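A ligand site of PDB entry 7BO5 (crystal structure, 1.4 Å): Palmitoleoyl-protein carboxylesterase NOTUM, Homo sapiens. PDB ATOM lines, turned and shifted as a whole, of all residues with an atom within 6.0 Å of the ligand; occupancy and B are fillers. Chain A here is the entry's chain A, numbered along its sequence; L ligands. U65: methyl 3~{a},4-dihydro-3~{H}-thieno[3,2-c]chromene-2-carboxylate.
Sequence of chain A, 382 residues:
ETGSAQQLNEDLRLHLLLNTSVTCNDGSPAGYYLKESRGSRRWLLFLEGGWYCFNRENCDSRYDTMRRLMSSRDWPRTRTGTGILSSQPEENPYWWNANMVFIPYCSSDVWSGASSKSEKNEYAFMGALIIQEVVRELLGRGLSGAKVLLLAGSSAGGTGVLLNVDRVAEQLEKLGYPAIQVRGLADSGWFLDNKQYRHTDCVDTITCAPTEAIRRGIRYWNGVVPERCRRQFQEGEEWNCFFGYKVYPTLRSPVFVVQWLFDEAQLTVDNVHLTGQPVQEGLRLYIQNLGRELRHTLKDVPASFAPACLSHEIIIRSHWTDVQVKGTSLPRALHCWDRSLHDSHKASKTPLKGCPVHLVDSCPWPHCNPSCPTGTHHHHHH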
ATOM      1  N   GLY A  49      14.736 -10.810 -17.105  1.00  0.00           N
ATOM      2  CA  GLY A  49      15.944 -10.631 -17.878  1.00  0.00           C
ATOM      3  C   GLY A  49      16.544 -11.944 -18.337  1.00  0.00           C
ATOM      4  O   GLY A  49      15.897 -12.997 -18.339  1.00  0.00           O
ATOM      5  N   GLY A  50      17.823 -11.880 -18.735  1.00  0.00           N
ATOM      6  CA  GLY A  50      18.509 -13.046 -19.247  1.00  0.00           C
ATOM      7  C   GLY A  50      19.221 -12.866 -20.577  1.00  0.00           C
ATOM      8  O   GLY A  50      19.019 -13.655 -21.519  1.00  0.00           O
ATOM      9  N   TRP A  51      20.081 -11.850 -20.675  1.00  0.00           N
ATOM     10  CA  TRP A  51      20.939 -11.633 -21.844  1.00  0.00           C
ATOM     11  C   TRP A  51      20.061 -11.378 -23.078  1.00  0.00           C
ATOM     12  O   TRP A  51      19.053 -10.666 -22.974  1.00  0.00           O
ATOM     13  CB  TRP A  51      22.001 -12.724 -22.003  1.00  0.00           C
ATOM     14  CG  TRP A  51      23.019 -12.701 -20.889  1.00  0.00           C
ATOM     15  CD1 TRP A  51      23.023 -13.485 -19.773  1.00  0.00           C
ATOM     16  CD2 TRP A  51      24.189 -11.877 -20.806  1.00  0.00           C
ATOM     17  NE1 TRP A  51      24.125 -13.205 -18.993  1.00  0.00           N
ATOM     18  CE2 TRP A  51      24.851 -12.212 -19.597  1.00  0.00           C
ATOM     19  CE3 TRP A  51      24.739 -10.886 -21.621  1.00  0.00           C
ATOM     20  CZ2 TRP A  51      26.029 -11.593 -19.196  1.00  0.00           C
ATOM     21  CZ3 TRP A  51      25.917 -10.267 -21.220  1.00  0.00           C
ATOM     22  CH2 TRP A  51      26.545 -10.625 -20.020  1.00  0.00           C
ATOM     23  N   TYR A  52      20.432 -11.911 -24.235  1.00  0.00           N
ATOM     24  CA  TYR A  52      19.873 -11.584 -25.546  1.00  0.00           C
ATOM     25  C   TYR A  52      20.641 -12.423 -26.560  1.00  0.00           C
ATOM     26  O   TYR A  52      21.628 -13.087 -26.219  1.00  0.00           O
ATOM     27  CB  TYR A  52      20.012 -10.087 -25.876  1.00  0.00           C
ATOM     28  CG  TYR A  52      21.400  -9.522 -25.579  1.00  0.00           C
ATOM     29  CD1 TYR A  52      22.469  -9.739 -26.440  1.00  0.00           C
ATOM     30  CD2 TYR A  52      21.628  -8.771 -24.425  1.00  0.00           C
ATOM     31  CE1 TYR A  52      23.725  -9.234 -26.159  1.00  0.00           C
ATOM     32  CE2 TYR A  52      22.883  -8.273 -24.138  1.00  0.00           C
ATOM     33  CZ  TYR A  52      23.936  -8.498 -25.006  1.00  0.00           C
ATOM     34  OH  TYR A  52      25.186  -7.994 -24.713  1.00  0.00           O
ATOM     35  N   TYR A 105      10.566 -13.303 -20.266  1.00  0.00           N
ATOM     36  CA  TYR A 105      11.399 -12.788 -21.333  1.00  0.00           C
ATOM     37  C   TYR A 105      11.602 -13.923 -22.333  1.00  0.00           C
ATOM     38  O   TYR A 105      12.331 -14.877 -22.066  1.00  0.00           O
ATOM     39  CB  TYR A 105      12.737 -12.389 -20.712  1.00  0.00           C
ATOM     40  CG  TYR A 105      13.761 -11.773 -21.625  1.00  0.00           C
ATOM     41  CD1 TYR A 105      13.410 -10.877 -22.642  1.00  0.00           C
ATOM     42  CD2 TYR A 105      15.109 -12.061 -21.432  1.00  0.00           C
ATOM     43  CE1 TYR A 105      14.391 -10.304 -23.445  1.00  0.00           C
ATOM     44  CE2 TYR A 105      16.091 -11.484 -22.218  1.00  0.00           C
ATOM     45  CZ  TYR A 105      15.732 -10.613 -23.217  1.00  0.00           C
ATOM     46  OH  TYR A 105      16.728 -10.052 -23.990  1.00  0.00           O
ATOM     47  N   VAL A 110      16.264  -7.600 -25.424  1.00  0.00           N
ATOM     48  CA  VAL A 110      16.294  -6.558 -24.411  1.00  0.00           C
ATOM     49  C   VAL A 110      14.972  -5.793 -24.414  1.00  0.00           C
ATOM     50  O   VAL A 110      14.913  -4.600 -24.099  1.00  0.00           O
ATOM     51  CB  VAL A 110      17.518  -5.624 -24.552  1.00  0.00           C
ATOM     52  CG1 VAL A 110      17.807  -4.881 -23.240  1.00  0.00           C
ATOM     53  CG2 VAL A 110      18.746  -6.426 -24.944  1.00  0.00           C
ATOM     54  N   SER A 154      14.546  -6.754 -14.225  1.00  0.00           N
ATOM     55  CA  SER A 154      15.905  -7.052 -13.794  1.00  0.00           C
ATOM     56  C   SER A 154      16.776  -7.429 -14.988  1.00  0.00           C
ATOM     57  O   SER A 154      16.327  -8.112 -15.903  1.00  0.00           O
ATOM     58  CB  SER A 154      15.918  -8.202 -12.775  1.00  0.00           C
ATOM     59  OG  SER A 154      15.293  -7.832 -11.556  1.00  0.00           O
ATOM     60  N   SER A 155      18.052  -7.004 -14.921  1.00  0.00           N
ATOM     61  CA  SER A 155      19.026  -7.226 -15.980  1.00  0.00           C
ATOM     62  C   SER A 155      18.524  -6.716 -17.323  1.00  0.00           C
ATOM     63  O   SER A 155      18.211  -5.534 -17.450  1.00  0.00           O
ATOM     64  CB  SER A 155      19.422  -8.710 -16.069  1.00  0.00           C
ATOM     65  OG  SER A 155      20.163  -9.083 -14.935  1.00  0.00           O
ATOM     66  N   ALA A 156      18.452  -7.598 -18.338  1.00  0.00           N
ATOM     67  CA  ALA A 156      17.875  -7.174 -19.612  1.00  0.00           C
ATOM     68  C   ALA A 156      16.455  -6.597 -19.422  1.00  0.00           C
ATOM     69  O   ALA A 156      16.052  -5.688 -20.167  1.00  0.00           O
ATOM     70  CB  ALA A 156      17.858  -8.333 -20.611  1.00  0.00           C
ATOM     71  N   GLY A 157      15.709  -7.091 -18.431  1.00  0.00           N
ATOM     72  CA  GLY A 157      14.420  -6.504 -18.119  1.00  0.00           C
ATOM     73  C   GLY A 157      14.511  -5.122 -17.500  1.00  0.00           C
ATOM     74  O   GLY A 157      13.608  -4.293 -17.682  1.00  0.00           O
ATOM     75  N   THR A 159      16.916  -2.909 -18.323  1.00  0.00           N
ATOM     76  CA  THR A 159      17.075  -2.081 -19.519  1.00  0.00           C
ATOM     77  C   THR A 159      15.747  -1.964 -20.258  1.00  0.00           C
ATOM     78  O   THR A 159      15.408  -0.890 -20.777  1.00  0.00           O
ATOM     79  CB  THR A 159      18.176  -2.646 -20.419  1.00  0.00           C
ATOM     80  OG1 THR A 159      19.356  -2.922 -19.640  1.00  0.00           O
ATOM     81  CG2 THR A 159      18.528  -1.651 -21.509  1.00  0.00           C
ATOM     82  N   SER A 188      19.500  -3.549 -12.180  1.00  0.00           N
ATOM     83  CA  SER A 188      20.637  -4.220 -12.821  1.00  0.00           C
ATOM     84  C   SER A 188      20.640  -4.073 -14.334  1.00  0.00           C
ATOM     85  O   SER A 188      21.158  -4.943 -15.050  1.00  0.00           O
ATOM     86  CB  SER A 188      20.710  -5.695 -12.425  1.00  0.00           C
ATOM     87  OG  SER A 188      20.913  -5.817 -11.036  1.00  0.00           O
ATOM     88  N   GLY A 189      20.079  -2.961 -14.833  1.00  0.00           N
ATOM     89  CA  GLY A 189      20.001  -2.729 -16.268  1.00  0.00           C
ATOM     90  C   GLY A 189      20.648  -1.436 -16.685  1.00  0.00           C
ATOM     91  O   GLY A 189      20.369  -0.930 -17.780  1.00  0.00           O
ATOM     92  N   PHE A 191      24.012  -0.040 -17.603  1.00  0.00           N
ATOM     93  CA  PHE A 191      25.325  -0.488 -18.057  1.00  0.00           C
ATOM     94  C   PHE A 191      26.149   0.674 -18.582  1.00  0.00           C
ATOM     95  O   PHE A 191      25.628   1.705 -19.007  1.00  0.00           O
ATOM     96  CB  PHE A 191      25.175  -1.554 -19.150  1.00  0.00           C
ATOM     97  CG  PHE A 191      24.529  -2.805 -18.652  1.00  0.00           C
ATOM     98  CD1 PHE A 191      23.177  -3.040 -18.857  1.00  0.00           C
ATOM     99  CD2 PHE A 191      25.260  -3.722 -17.923  1.00  0.00           C
ATOM    100  CE1 PHE A 191      22.576  -4.180 -18.363  1.00  0.00           C
ATOM    101  CE2 PHE A 191      24.659  -4.869 -17.421  1.00  0.00           C
ATOM    102  CZ  PHE A 191      23.305  -5.094 -17.658  1.00  0.00           C
ATOM    103  N   PRO A 210      29.272  -4.842 -25.596  1.00  0.00           N
ATOM    104  CA  PRO A 210      27.856  -4.427 -25.601  1.00  0.00           C
ATOM    105  C   PRO A 210      27.482  -3.435 -26.693  1.00  0.00           C
ATOM    106  O   PRO A 210      26.415  -3.567 -27.291  1.00  0.00           O
ATOM    107  CB  PRO A 210      27.652  -3.837 -24.195  1.00  0.00           C
ATOM    108  CG  PRO A 210      28.736  -4.428 -23.371  1.00  0.00           C
ATOM    109  CD  PRO A 210      29.906  -4.595 -24.292  1.00  0.00           C
ATOM    110  N   ILE A 214      24.644  -4.677 -29.335  1.00  0.00           N
ATOM    111  CA  ILE A 214      23.355  -3.990 -29.452  1.00  0.00           C
ATOM    112  C   ILE A 214      23.201  -3.349 -30.817  1.00  0.00           C
ATOM    113  O   ILE A 214      22.108  -3.327 -31.394  1.00  0.00           O
ATOM    114  CB  ILE A 214      23.194  -3.002 -28.288  1.00  0.00           C
ATOM    115  CG1 ILE A 214      22.984  -3.770 -26.995  1.00  0.00           C
ATOM    116  CG2 ILE A 214      22.029  -2.053 -28.527  1.00  0.00           C
ATOM    117  CD1 ILE A 214      23.673  -3.157 -25.852  1.00  0.00           C
ATOM    118  N   PHE A 242      20.229   2.231 -25.363  1.00  0.00           N
ATOM    119  CA  PHE A 242      20.224   1.073 -24.476  1.00  0.00           C
ATOM    120  C   PHE A 242      21.084   1.299 -23.243  1.00  0.00           C
ATOM    121  O   PHE A 242      21.101   0.438 -22.350  1.00  0.00           O
ATOM    122  CB  PHE A 242      20.744  -0.178 -25.209  1.00  0.00           C
ATOM    123  CG  PHE A 242      19.754  -0.787 -26.161  1.00  0.00           C
ATOM    124  CD1 PHE A 242      19.289  -0.068 -27.264  1.00  0.00           C
ATOM    125  CD2 PHE A 242      19.315  -2.092 -25.985  1.00  0.00           C
ATOM    126  CE1 PHE A 242      18.404  -0.649 -28.159  1.00  0.00           C
ATOM    127  CE2 PHE A 242      18.422  -2.671 -26.891  1.00  0.00           C
ATOM    128  CZ  PHE A 242      17.968  -1.944 -27.974  1.00  0.00           C
ATOM    129  N   PHE A 243      21.787   2.426 -23.156  1.00  0.00           N
ATOM    130  CA  PHE A 243      22.671   2.711 -22.031  1.00  0.00           C
ATOM    131  C   PHE A 243      21.993   3.687 -21.093  1.00  0.00           C
ATOM    132  O   PHE A 243      21.710   4.834 -21.473  1.00  0.00           O
ATOM    133  CB  PHE A 243      24.037   3.156 -22.521  1.00  0.00           C
ATOM    134  CG  PHE A 243      24.790   2.043 -23.147  1.00  0.00           C
ATOM    135  CD1 PHE A 243      24.564   1.691 -24.461  1.00  0.00           C
ATOM    136  CD2 PHE A 243      25.630   1.249 -22.369  1.00  0.00           C
ATOM    137  CE1 PHE A 243      25.207   0.616 -25.025  1.00  0.00           C
ATOM    138  CE2 PHE A 243      26.287   0.165 -22.928  1.00  0.00           C
ATOM    139  CZ  PHE A 243      26.065  -0.156 -24.253  1.00  0.00           C
ATOM    140  N   ALA A 265      27.320  -8.860 -14.567  1.00  0.00           N
ATOM    141  CA  ALA A 265      27.163  -8.867 -16.022  1.00  0.00           C
ATOM    142  C   ALA A 265      28.012  -7.780 -16.672  1.00  0.00           C
ATOM    143  O   ALA A 265      28.603  -8.006 -17.741  1.00  0.00           O
ATOM    144  CB  ALA A 265      25.692  -8.728 -16.412  1.00  0.00           C
ATOM    145  N   GLN A 266      28.097  -6.607 -16.030  1.00  0.00           N
ATOM    146  CA  GLN A 266      29.005  -5.563 -16.485  1.00  0.00           C
ATOM    147  C   GLN A 266      30.449  -6.061 -16.503  1.00  0.00           C
ATOM    148  O   GLN A 266      31.184  -5.863 -17.472  1.00  0.00           O
ATOM    149  CB  GLN A 266      28.862  -4.330 -15.584  1.00  0.00           C
ATOM    150  CG  GLN A 266      29.810  -3.187 -15.945  1.00  0.00           C
ATOM    151  CD  GLN A 266      29.339  -2.389 -17.140  1.00  0.00           C
ATOM    152  OE1 GLN A 266      28.196  -1.941 -17.191  1.00  0.00           O
ATOM    153  NE2 GLN A 266      30.232  -2.192 -18.107  1.00  0.00           N
ATOM    154  N   VAL A 269      31.013  -8.636 -19.477  1.00  0.00           N
ATOM    155  CA  VAL A 269      31.224  -8.001 -20.786  1.00  0.00           C
ATOM    156  C   VAL A 269      32.521  -7.207 -20.810  1.00  0.00           C
ATOM    157  O   VAL A 269      33.075  -6.970 -21.897  1.00  0.00           O
ATOM    158  CB  VAL A 269      30.006  -7.183 -21.259  1.00  0.00           C
ATOM    159  CG1 VAL A 269      28.801  -8.085 -21.418  1.00  0.00           C
ATOM    160  CG2 VAL A 269      29.704  -6.050 -20.304  1.00  0.00           C
ATOM    161  N   HIS A 312      24.522  -9.719  -8.853  1.00  0.00           N
ATOM    162  CA  HIS A 312      23.731  -9.628 -10.074  1.00  0.00           C
ATOM    163  C   HIS A 312      22.244  -9.763  -9.774  1.00  0.00           C
ATOM    164  O   HIS A 312      21.819 -10.773  -9.223  1.00  0.00           O
ATOM    165  CB  HIS A 312      24.142 -10.712 -11.078  1.00  0.00           C
ATOM    166  CG  HIS A 312      23.407 -10.607 -12.381  1.00  0.00           C
ATOM    167  ND1 HIS A 312      22.623 -11.619 -12.870  1.00  0.00           N
ATOM    168  CD2 HIS A 312      23.301  -9.580 -13.256  1.00  0.00           C
ATOM    169  CE1 HIS A 312      22.091 -11.236 -14.018  1.00  0.00           C
ATOM    170  NE2 HIS A 312      22.487 -10.007 -14.280  1.00  0.00           N
ATOM    171  N   GLU A 313      21.468  -8.756 -10.199  1.00  0.00           N
ATOM    172  CA  GLU A 313      20.031  -8.644  -9.954  1.00  0.00           C
ATOM    173  C   GLU A 313      19.721  -8.568  -8.457  1.00  0.00           C
ATOM    174  O   GLU A 313      20.596  -8.847  -7.645  1.00  0.00           O
ATOM    175  CB  GLU A 313      19.226  -9.771 -10.608  1.00  0.00           C
ATOM    176  CG  GLU A 313      19.203  -9.711 -12.106  1.00  0.00           C
ATOM    177  CD  GLU A 313      18.505 -10.906 -12.739  1.00  0.00           C
ATOM    178  OE1 GLU A 313      18.249 -11.884 -12.016  1.00  0.00           O
ATOM    179  OE2 GLU A 313      18.224 -10.859 -13.966  1.00  0.00           O
HETATM  180  C01 U65 L   1      22.050 -11.117 -17.401  1.00  0.00           C
HETATM  181  C03 U65 L   1      21.850  -9.407 -18.981  1.00  0.00           C
HETATM  182  C05 U65 L   1      22.451  -8.229 -19.714  1.00  0.00           C
HETATM  183  C06 U65 L   1      23.769  -7.944 -19.917  1.00  0.00           C
HETATM  184  C07 U65 L   1      24.014  -6.747 -20.639  1.00  0.00           C
HETATM  185  C08 U65 L   1      25.429  -6.243 -20.963  1.00  0.00           C
HETATM  186  C10 U65 L   1      24.250  -4.279 -21.880  1.00  0.00           C
HETATM  187  C11 U65 L   1      24.331  -2.993 -22.452  1.00  0.00           C
HETATM  188  C12 U65 L   1      23.168  -2.284 -22.752  1.00  0.00           C
HETATM  189  C13 U65 L   1      21.927  -2.870 -22.503  1.00  0.00           C
HETATM  190  C14 U65 L   1      21.840  -4.136 -21.940  1.00  0.00           C
HETATM  191  C15 U65 L   1      23.027  -4.863 -21.669  1.00  0.00           C
HETATM  192  C16 U65 L   1      22.928  -6.071 -21.038  1.00  0.00           C
HETATM  193  O02 U65 L   1      22.706 -10.134 -18.153  1.00  0.00           O
HETATM  194  O04 U65 L   1      20.690  -9.634 -19.038  1.00  0.00           O
HETATM  195  O09 U65 L   1      25.491  -4.954 -21.574  1.00  0.00           O
HETATM  196  S17 U65 L   1      21.564  -6.984 -20.453  1.00  0.00           S
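Gly 50 touches the ligand. Tyr 52 touches the ligand. Ser 155 touches the ligand (CB to O04, 3.4 Å). OG1 of Thr 159 touches C14 of the ligand, at 3.6 Å. CE1 of Phe 191 touches C16 of the ligand, 3.3 Å away. CB of Pro 210 touches O09 of the ligand (3.6 Å). Ile 214 touches the ligand. O of Phe 242 touches C13 of the ligand (3.4 Å). Phe 243 touches the ligand (CE2 to C11, 3.7 Å). Ala 265 touches the ligand. CG1 of Val 269 touches C08 of the ligand (3.9 Å). His 312 touches the ligand. Hydrophobic or aromatic side chains within 4 Å of the ligand: Trp 51, Tyr 52, Ala 156, Phe 191, Pro 210, Ile 214, Phe 242, Phe 243, Ala 265, Val 269 and His 312. Of the 23 residues printed, 14 come within 4 Å of the ligand. Along chain A the residues within 4 Å of the ligand span positions 50 to 312.
The backbone NH (N) of Trp 51 lies within hydrogen-bond range of an oxygen (O04) of the ligand (2.8 Å). The backbone NH (N) of Ala 156 lies within hydrogen-bond range of an oxygen (O04) of the ligand (3.1 Å). NE1 of Trp 51 sits close to O02 of the ligand (3.5 Å).
OE2 of Glu 313 lies within hydrogen-bond range of OG of Ser 155 (2.8 Å). OG1 of Thr 159 is in hydrogen-bond range of O of Gly 189. The backbone carbonyl oxygen (O) of Trp 51 lies within hydrogen-bond range of the side-chain hydroxyl (OH) of Tyr 105 (2.6 Å). OG of Ser 155 is in hydrogen-bond range of NE2 of His 312 (2.6 Å).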
